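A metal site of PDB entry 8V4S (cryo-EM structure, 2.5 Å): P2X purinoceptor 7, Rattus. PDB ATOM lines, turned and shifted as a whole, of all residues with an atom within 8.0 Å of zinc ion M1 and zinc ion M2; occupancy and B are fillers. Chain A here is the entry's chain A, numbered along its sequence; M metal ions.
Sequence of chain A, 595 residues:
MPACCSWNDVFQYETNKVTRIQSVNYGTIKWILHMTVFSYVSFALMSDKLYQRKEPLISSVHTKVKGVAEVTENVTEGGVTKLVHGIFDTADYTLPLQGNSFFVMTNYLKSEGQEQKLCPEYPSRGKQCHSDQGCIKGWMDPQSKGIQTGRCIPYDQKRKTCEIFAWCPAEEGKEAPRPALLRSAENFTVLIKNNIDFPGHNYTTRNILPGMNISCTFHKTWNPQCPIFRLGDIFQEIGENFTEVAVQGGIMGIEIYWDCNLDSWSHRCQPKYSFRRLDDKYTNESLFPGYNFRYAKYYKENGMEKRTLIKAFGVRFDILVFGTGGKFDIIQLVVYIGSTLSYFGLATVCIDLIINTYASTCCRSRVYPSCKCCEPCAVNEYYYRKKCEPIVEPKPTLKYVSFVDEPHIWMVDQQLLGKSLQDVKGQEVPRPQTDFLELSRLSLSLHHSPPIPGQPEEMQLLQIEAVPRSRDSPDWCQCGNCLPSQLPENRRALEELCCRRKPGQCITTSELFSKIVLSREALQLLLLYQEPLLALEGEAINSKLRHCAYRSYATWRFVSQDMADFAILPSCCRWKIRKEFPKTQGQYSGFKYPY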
ATOM      1  N   VAL A 404      17.293  14.616  -4.022  1.00  0.00           N
ATOM      2  CA  VAL A 404      17.744  14.972  -5.360  1.00  0.00           C
ATOM      3  C   VAL A 404      18.512  13.835  -6.005  1.00  0.00           C
ATOM      4  O   VAL A 404      18.538  13.705  -7.237  1.00  0.00           O
ATOM      5  CB  VAL A 404      18.582  16.279  -5.315  1.00  0.00           C
ATOM      6  CG1 VAL A 404      19.923  16.036  -4.636  1.00  0.00           C
ATOM      7  CG2 VAL A 404      18.771  16.833  -6.714  1.00  0.00           C
ATOM      8  N   GLN A 422      15.567  11.910   8.403  1.00  0.00           N
ATOM      9  CA  GLN A 422      16.410  11.406   7.338  1.00  0.00           C
ATOM     10  C   GLN A 422      16.466   9.877   7.333  1.00  0.00           C
ATOM     11  O   GLN A 422      16.391   9.251   6.266  1.00  0.00           O
ATOM     12  CB  GLN A 422      17.819  11.982   7.476  1.00  0.00           C
ATOM     13  CG  GLN A 422      18.766  11.589   6.352  1.00  0.00           C
ATOM     14  CD  GLN A 422      18.588  12.451   5.127  1.00  0.00           C
ATOM     15  OE1 GLN A 422      17.823  13.412   5.131  1.00  0.00           O
ATOM     16  NE2 GLN A 422      19.305  12.118   4.063  1.00  0.00           N
ATOM     17  N   SER A 473      29.113  19.761   9.392  1.00  0.00           N
ATOM     18  CA  SER A 473      27.770  19.374   9.005  1.00  0.00           C
ATOM     19  C   SER A 473      27.228  18.299   9.940  1.00  0.00           C
ATOM     20  O   SER A 473      27.994  17.525  10.524  1.00  0.00           O
ATOM     21  CB  SER A 473      27.750  18.867   7.561  1.00  0.00           C
ATOM     22  OG  SER A 473      28.508  17.680   7.435  1.00  0.00           O
ATOM     23  N   PRO A 474      25.910  18.231  10.110  1.00  0.00           N
ATOM     24  CA  PRO A 474      25.329  17.199  10.991  1.00  0.00           C
ATOM     25  C   PRO A 474      25.596  15.800  10.461  1.00  0.00           C
ATOM     26  O   PRO A 474      25.968  15.597   9.306  1.00  0.00           O
ATOM     27  CB  PRO A 474      23.829  17.522  10.971  1.00  0.00           C
ATOM     28  CG  PRO A 474      23.751  18.960  10.584  1.00  0.00           C
ATOM     29  CD  PRO A 474      24.891  19.183   9.638  1.00  0.00           C
ATOM     30  N   TRP A 476      23.468  13.438   9.929  1.00  0.00           N
ATOM     31  CA  TRP A 476      22.470  13.056   8.940  1.00  0.00           C
ATOM     32  C   TRP A 476      22.538  13.872   7.661  1.00  0.00           C
ATOM     33  O   TRP A 476      21.706  13.683   6.770  1.00  0.00           O
ATOM     34  CB  TRP A 476      21.066  13.165   9.543  1.00  0.00           C
ATOM     35  CG  TRP A 476      20.850  14.419  10.344  1.00  0.00           C
ATOM     36  CD1 TRP A 476      20.888  14.531  11.707  1.00  0.00           C
ATOM     37  CD2 TRP A 476      20.562  15.722   9.846  1.00  0.00           C
ATOM     38  NE1 TRP A 476      20.644  15.828  12.081  1.00  0.00           N
ATOM     39  CE2 TRP A 476      20.436  16.582  10.950  1.00  0.00           C
ATOM     40  CE3 TRP A 476      20.391  16.254   8.561  1.00  0.00           C
ATOM     41  CZ2 TRP A 476      20.148  17.933  10.820  1.00  0.00           C
ATOM     42  CZ3 TRP A 476      20.109  17.597   8.430  1.00  0.00           C
ATOM     43  CH2 TRP A 476      19.992  18.422   9.553  1.00  0.00           C
ATOM     44  N   CYS A 477      23.502  14.794   7.549  1.00  0.00           N
ATOM     45  CA  CYS A 477      23.633  15.647   6.377  1.00  0.00           C
ATOM     46  C   CYS A 477      24.663  15.060   5.426  1.00  0.00           C
ATOM     47  O   CYS A 477      25.825  14.868   5.805  1.00  0.00           O
ATOM     48  CB  CYS A 477      24.031  17.063   6.786  1.00  0.00           C
ATOM     49  SG  CYS A 477      24.450  18.120   5.377  1.00  0.00           S
ATOM     50  N   GLN A 478      24.242  14.772   4.199  1.00  0.00           N
ATOM     51  CA  GLN A 478      25.110  14.233   3.160  1.00  0.00           C
ATOM     52  C   GLN A 478      25.496  15.283   2.118  1.00  0.00           C
ATOM     53  O   GLN A 478      26.083  14.939   1.094  1.00  0.00           O
ATOM     54  CB  GLN A 478      24.451  13.045   2.484  1.00  0.00           C
ATOM     55  CG  GLN A 478      24.723  11.702   3.151  1.00  0.00           C
ATOM     56  CD  GLN A 478      23.752  11.409   4.288  1.00  0.00           C
ATOM     57  OE1 GLN A 478      23.513  12.249   5.151  1.00  0.00           O
ATOM     58  NE2 GLN A 478      23.193  10.201   4.287  1.00  0.00           N
ATOM     59  N   CYS A 479      25.161  16.564   2.350  1.00  0.00           N
ATOM     60  CA  CYS A 479      25.509  17.629   1.428  1.00  0.00           C
ATOM     61  C   CYS A 479      26.416  18.684   2.022  1.00  0.00           C
ATOM     62  O   CYS A 479      27.108  19.369   1.263  1.00  0.00           O
ATOM     63  CB  CYS A 479      24.242  18.301   0.880  1.00  0.00           C
ATOM     64  SG  CYS A 479      23.353  19.359   2.048  1.00  0.00           S
ATOM     65  N   GLY A 480      26.429  18.860   3.347  1.00  0.00           N
ATOM     66  CA  GLY A 480      27.333  19.783   3.998  1.00  0.00           C
ATOM     67  C   GLY A 480      26.762  21.164   4.249  1.00  0.00           C
ATOM     68  O   GLY A 480      27.309  21.885   5.092  1.00  0.00           O
ATOM     69  N   ASN A 481      25.696  21.553   3.553  1.00  0.00           N
ATOM     70  CA  ASN A 481      25.101  22.869   3.751  1.00  0.00           C
ATOM     71  C   ASN A 481      23.982  22.863   4.786  1.00  0.00           C
ATOM     72  O   ASN A 481      23.484  23.932   5.135  1.00  0.00           O
ATOM     73  CB  ASN A 481      24.569  23.405   2.414  1.00  0.00           C
ATOM     74  CG  ASN A 481      24.416  24.918   2.411  1.00  0.00           C
ATOM     75  OD1 ASN A 481      23.347  25.439   2.727  1.00  0.00           O
ATOM     76  ND2 ASN A 481      25.486  25.623   2.067  1.00  0.00           N
ATOM     77  N   CYS A 482      23.588  21.692   5.281  1.00  0.00           N
ATOM     78  CA  CYS A 482      22.528  21.624   6.274  1.00  0.00           C
ATOM     79  C   CYS A 482      23.022  22.154   7.619  1.00  0.00           C
ATOM     80  O   CYS A 482      24.221  22.126   7.921  1.00  0.00           O
ATOM     81  CB  CYS A 482      22.039  20.186   6.431  1.00  0.00           C
ATOM     82  SG  CYS A 482      21.001  19.588   5.080  1.00  0.00           S
ATOM     83  N   LEU A 483      22.082  22.643   8.420  1.00  0.00           N
ATOM     84  CA  LEU A 483      22.373  23.205   9.728  1.00  0.00           C
ATOM     85  C   LEU A 483      21.513  22.553  10.791  1.00  0.00           C
ATOM     86  O   LEU A 483      20.416  22.071  10.495  1.00  0.00           O
ATOM     87  CB  LEU A 483      22.144  24.716   9.742  1.00  0.00           C
ATOM     88  CG  LEU A 483      22.942  25.567   8.757  1.00  0.00           C
ATOM     89  CD1 LEU A 483      22.678  27.042   8.986  1.00  0.00           C
ATOM     90  CD2 LEU A 483      24.431  25.262   8.850  1.00  0.00           C
ATOM     91  N   LEU A 497      16.453  16.724   8.158  1.00  0.00           N
ATOM     92  CA  LEU A 497      16.331  16.095   6.845  1.00  0.00           C
ATOM     93  C   LEU A 497      17.353  16.708   5.900  1.00  0.00           C
ATOM     94  O   LEU A 497      17.617  17.907   5.948  1.00  0.00           O
ATOM     95  CB  LEU A 497      14.915  16.271   6.278  1.00  0.00           C
ATOM     96  CG  LEU A 497      14.594  15.596   4.941  1.00  0.00           C
ATOM     97  CD1 LEU A 497      14.521  14.090   5.098  1.00  0.00           C
ATOM     98  CD2 LEU A 497      13.293  16.148   4.375  1.00  0.00           C
ATOM     99  N   CYS A 498      17.919  15.869   5.034  1.00  0.00           N
ATOM    100  CA  CYS A 498      18.906  16.298   4.053  1.00  0.00           C
ATOM    101  C   CYS A 498      18.313  16.182   2.653  1.00  0.00           C
ATOM    102  O   CYS A 498      17.351  15.447   2.419  1.00  0.00           O
ATOM    103  CB  CYS A 498      20.199  15.480   4.150  1.00  0.00           C
ATOM    104  SG  CYS A 498      21.647  16.255   3.399  1.00  0.00           S
ATOM    105  N   CYS A 499      18.915  16.898   1.708  1.00  0.00           N
ATOM    106  CA  CYS A 499      18.441  16.918   0.338  1.00  0.00           C
ATOM    107  C   CYS A 499      18.815  15.663  -0.438  1.00  0.00           C
ATOM    108  O   CYS A 499      18.283  15.460  -1.540  1.00  0.00           O
ATOM    109  CB  CYS A 499      18.981  18.145  -0.398  1.00  0.00           C
ATOM    110  SG  CYS A 499      20.775  18.247  -0.462  1.00  0.00           S
ATOM    111  N   ARG A 500      19.717  14.842   0.086  1.00  0.00           N
ATOM    112  CA  ARG A 500      20.179  13.650  -0.609  1.00  0.00           C
ATOM    113  C   ARG A 500      20.451  12.544   0.398  1.00  0.00           C
ATOM    114  O   ARG A 500      20.795  12.818   1.551  1.00  0.00           O
ATOM    115  CB  ARG A 500      21.430  13.936  -1.439  1.00  0.00           C
ATOM    116  CG  ARG A 500      22.377  14.935  -0.781  1.00  0.00           C
ATOM    117  CD  ARG A 500      23.674  15.121  -1.566  1.00  0.00           C
ATOM    118  NE  ARG A 500      23.475  15.242  -3.003  1.00  0.00           N
ATOM    119  CZ  ARG A 500      23.724  14.266  -3.874  1.00  0.00           C
ATOM    120  NH1 ARG A 500      24.186  13.097  -3.452  1.00  0.00           N
ATOM    121  NH2 ARG A 500      23.512  14.459  -5.168  1.00  0.00           N
ATOM    122  N   GLY A 504      27.308  14.008  -1.849  1.00  0.00           N
ATOM    123  CA  GLY A 504      27.404  14.614  -3.167  1.00  0.00           C
ATOM    124  C   GLY A 504      27.105  16.097  -3.095  1.00  0.00           C
ATOM    125  O   GLY A 504      27.142  16.704  -2.028  1.00  0.00           O
ATOM    126  N   GLN A 505      26.818  16.670  -4.263  1.00  0.00           N
ATOM    127  CA  GLN A 505      26.512  18.081  -4.361  1.00  0.00           C
ATOM    128  C   GLN A 505      25.131  18.386  -3.780  1.00  0.00           C
ATOM    129  O   GLN A 505      24.246  17.532  -3.761  1.00  0.00           O
ATOM    130  CB  GLN A 505      26.582  18.554  -5.811  1.00  0.00           C
ATOM    131  CG  GLN A 505      26.038  17.541  -6.808  1.00  0.00           C
ATOM    132  CD  GLN A 505      26.177  18.004  -8.243  1.00  0.00           C
ATOM    133  OE1 GLN A 505      26.161  19.202  -8.532  1.00  0.00           O
ATOM    134  NE2 GLN A 505      26.309  17.054  -9.160  1.00  0.00           N
ATOM    135  N   CYS A 506      24.965  19.613  -3.297  1.00  0.00           N
ATOM    136  CA  CYS A 506      23.711  20.038  -2.710  1.00  0.00           C
ATOM    137  C   CYS A 506      22.761  20.571  -3.776  1.00  0.00           C
ATOM    138  O   CYS A 506      23.195  21.043  -4.838  1.00  0.00           O
ATOM    139  CB  CYS A 506      23.949  21.123  -1.646  1.00  0.00           C
ATOM    140  SG  CYS A 506      22.463  21.681  -0.806  1.00  0.00           S
ATOM    141  N   ILE A 507      21.465  20.479  -3.498  1.00  0.00           N
ATOM    142  CA  ILE A 507      20.454  20.989  -4.406  1.00  0.00           C
ATOM    143  C   ILE A 507      20.555  22.501  -4.539  1.00  0.00           C
ATOM    144  O   ILE A 507      20.316  23.062  -5.615  1.00  0.00           O
ATOM    145  CB  ILE A 507      19.052  20.551  -3.946  1.00  0.00           C
ATOM    146  CG1 ILE A 507      17.959  21.122  -4.848  1.00  0.00           C
ATOM    147  CG2 ILE A 507      18.815  20.945  -2.511  1.00  0.00           C
ATOM    148  CD1 ILE A 507      17.749  20.345  -6.114  1.00  0.00           C
ATOM    149  N   THR A 508      20.914  23.196  -3.457  1.00  0.00           N
ATOM    150  CA  THR A 508      20.987  24.652  -3.468  1.00  0.00           C
ATOM    151  C   THR A 508      22.062  25.176  -4.411  1.00  0.00           C
ATOM    152  O   THR A 508      22.009  26.344  -4.794  1.00  0.00           O
ATOM    153  CB  THR A 508      21.234  25.187  -2.057  1.00  0.00           C
ATOM    154  OG1 THR A 508      22.430  24.589  -1.527  1.00  0.00           O
ATOM    155  CG2 THR A 508      20.064  24.864  -1.152  1.00  0.00           C
ATOM    156  N   THR A 509      23.037  24.346  -4.786  1.00  0.00           N
ATOM    157  CA  THR A 509      24.116  24.796  -5.655  1.00  0.00           C
ATOM    158  C   THR A 509      23.640  25.062  -7.076  1.00  0.00           C
ATOM    159  O   THR A 509      24.288  25.823  -7.798  1.00  0.00           O
ATOM    160  CB  THR A 509      25.250  23.769  -5.679  1.00  0.00           C
ATOM    161  OG1 THR A 509      24.791  22.559  -6.297  1.00  0.00           O
ATOM    162  CG2 THR A 509      25.709  23.462  -4.253  1.00  0.00           C
ATOM    163  N   TYR A 553       9.580  25.942  -3.555  1.00  0.00           N
ATOM    164  CA  TYR A 553      10.411  24.738  -3.513  1.00  0.00           C
ATOM    165  C   TYR A 553       9.550  23.488  -3.453  1.00  0.00           C
ATOM    166  O   TYR A 553       9.834  22.498  -4.136  1.00  0.00           O
ATOM    167  CB  TYR A 553      11.367  24.786  -2.316  1.00  0.00           C
ATOM    168  CG  TYR A 553      12.210  23.528  -2.203  1.00  0.00           C
ATOM    169  CD1 TYR A 553      13.408  23.414  -2.883  1.00  0.00           C
ATOM    170  CD2 TYR A 553      11.801  22.459  -1.422  1.00  0.00           C
ATOM    171  CE1 TYR A 553      14.175  22.266  -2.787  1.00  0.00           C
ATOM    172  CE2 TYR A 553      12.557  21.313  -1.314  1.00  0.00           C
ATOM    173  CZ  TYR A 553      13.746  21.219  -2.002  1.00  0.00           C
ATOM    174  OH  TYR A 553      14.507  20.079  -1.906  1.00  0.00           O
ATOM    175  N   PRO A 570      14.293  20.169   3.210  1.00  0.00           N
ATOM    176  CA  PRO A 570      15.546  19.824   3.882  1.00  0.00           C
ATOM    177  C   PRO A 570      16.172  21.036   4.565  1.00  0.00           C
ATOM    178  O   PRO A 570      15.834  22.183   4.279  1.00  0.00           O
ATOM    179  CB  PRO A 570      16.437  19.307   2.745  1.00  0.00           C
ATOM    180  CG  PRO A 570      15.844  19.867   1.513  1.00  0.00           C
ATOM    181  CD  PRO A 570      14.373  19.989   1.752  1.00  0.00           C
ATOM    182  N   SER A 571      17.081  20.753   5.498  1.00  0.00           N
ATOM    183  CA  SER A 571      17.648  21.813   6.323  1.00  0.00           C
ATOM    184  C   SER A 571      18.442  22.807   5.497  1.00  0.00           C
ATOM    185  O   SER A 571      18.417  24.015   5.775  1.00  0.00           O
ATOM    186  CB  SER A 571      18.520  21.208   7.420  1.00  0.00           C
ATOM    187  OG  SER A 571      17.731  20.540   8.386  1.00  0.00           O
ATOM    188  N   CYS A 572      19.166  22.327   4.479  1.00  0.00           N
ATOM    189  CA  CYS A 572      19.977  23.229   3.663  1.00  0.00           C
ATOM    190  C   CYS A 572      19.115  24.272   2.957  1.00  0.00           C
ATOM    191  O   CYS A 572      19.388  25.473   3.043  1.00  0.00           O
ATOM    192  CB  CYS A 572      20.787  22.410   2.648  1.00  0.00           C
ATOM    193  SG  CYS A 572      19.869  21.070   1.873  1.00  0.00           S
ATOM    194  N   CYS A 573      18.068  23.816   2.259  1.00  0.00           N
ATOM    195  CA  CYS A 573      17.181  24.741   1.574  1.00  0.00           C
ATOM    196  C   CYS A 573      16.472  25.665   2.551  1.00  0.00           C
ATOM    197  O   CYS A 573      16.353  26.872   2.316  1.00  0.00           O
ATOM    198  CB  CYS A 573      16.148  23.972   0.751  1.00  0.00           C
ATOM    199  SG  CYS A 573      16.853  22.731  -0.337  1.00  0.00           S
HETATM  200 ZN    ZN M   1      21.621  20.093   0.670  1.00  0.00          ZN
HETATM  201 ZN    ZN M   2      22.600  18.306   3.975  1.00  0.00          ZN
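The backbone carbonyl oxygen (O) of Gln 478 sits at hydrogen-bond distance from the backbone NH (N) of Gly 504, 3.3 Å away. N of Gly 480 sits close to SG of Cys 477 (2.9 Å). O of Cys 506 is in hydrogen-bond range of OG1 of Thr 509, at 2.6 Å. N of Asn 481 sits close to SG of Cys 479 (3.5 Å). The side-chain amide oxygen (OE1) of Gln 478 lies close to the backbone carbonyl oxygen (O) of Trp 476. The backbone NH (N) of Cys 572 lies close to the side-chain sulfur (SG) of Cys 482 (3.4 Å). The side-chain hydroxyl (OG1) of Thr 508 lies close to the side-chain sulfur (SG) of Cys 506 (3.0 Å). The backbone NH (N) of Cys 498 is in hydrogen-bond range of the side-chain amide oxygen (OE1) of Gln 422, at 2.5 Å.
Within 4 Å of zinc ion M1: Cys 479, Cys 499, Cys 506 and Cys 572. Along chain A the residues within 4 Å of zinc ion M1 span positions 479 to 572.
Merely in contact with zinc ion M2: Gln 478 (3.9 Å) and Gly 480 (3.9 Å).
Zinc ion M1 is bound by SG of Cys 499 (2.3 Å), SG of Cys 506 (2.3 Å), SG of Cys 479 (2.3 Å) and SG of Cys 572 (2.3 Å). Zinc ion M1 has four donor atoms within binding distance.
Zinc ion M2 is bound by SG of Cys 479, at 2.3 Å. The side-chain sulfur (SG) of Cys 482 is bound to zinc ion M2, 2.3 Å away. Zinc ion M2 is bound by SG of Cys 477. Zinc ion M2 is bound by SG of Cys 498 (2.3 Å).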
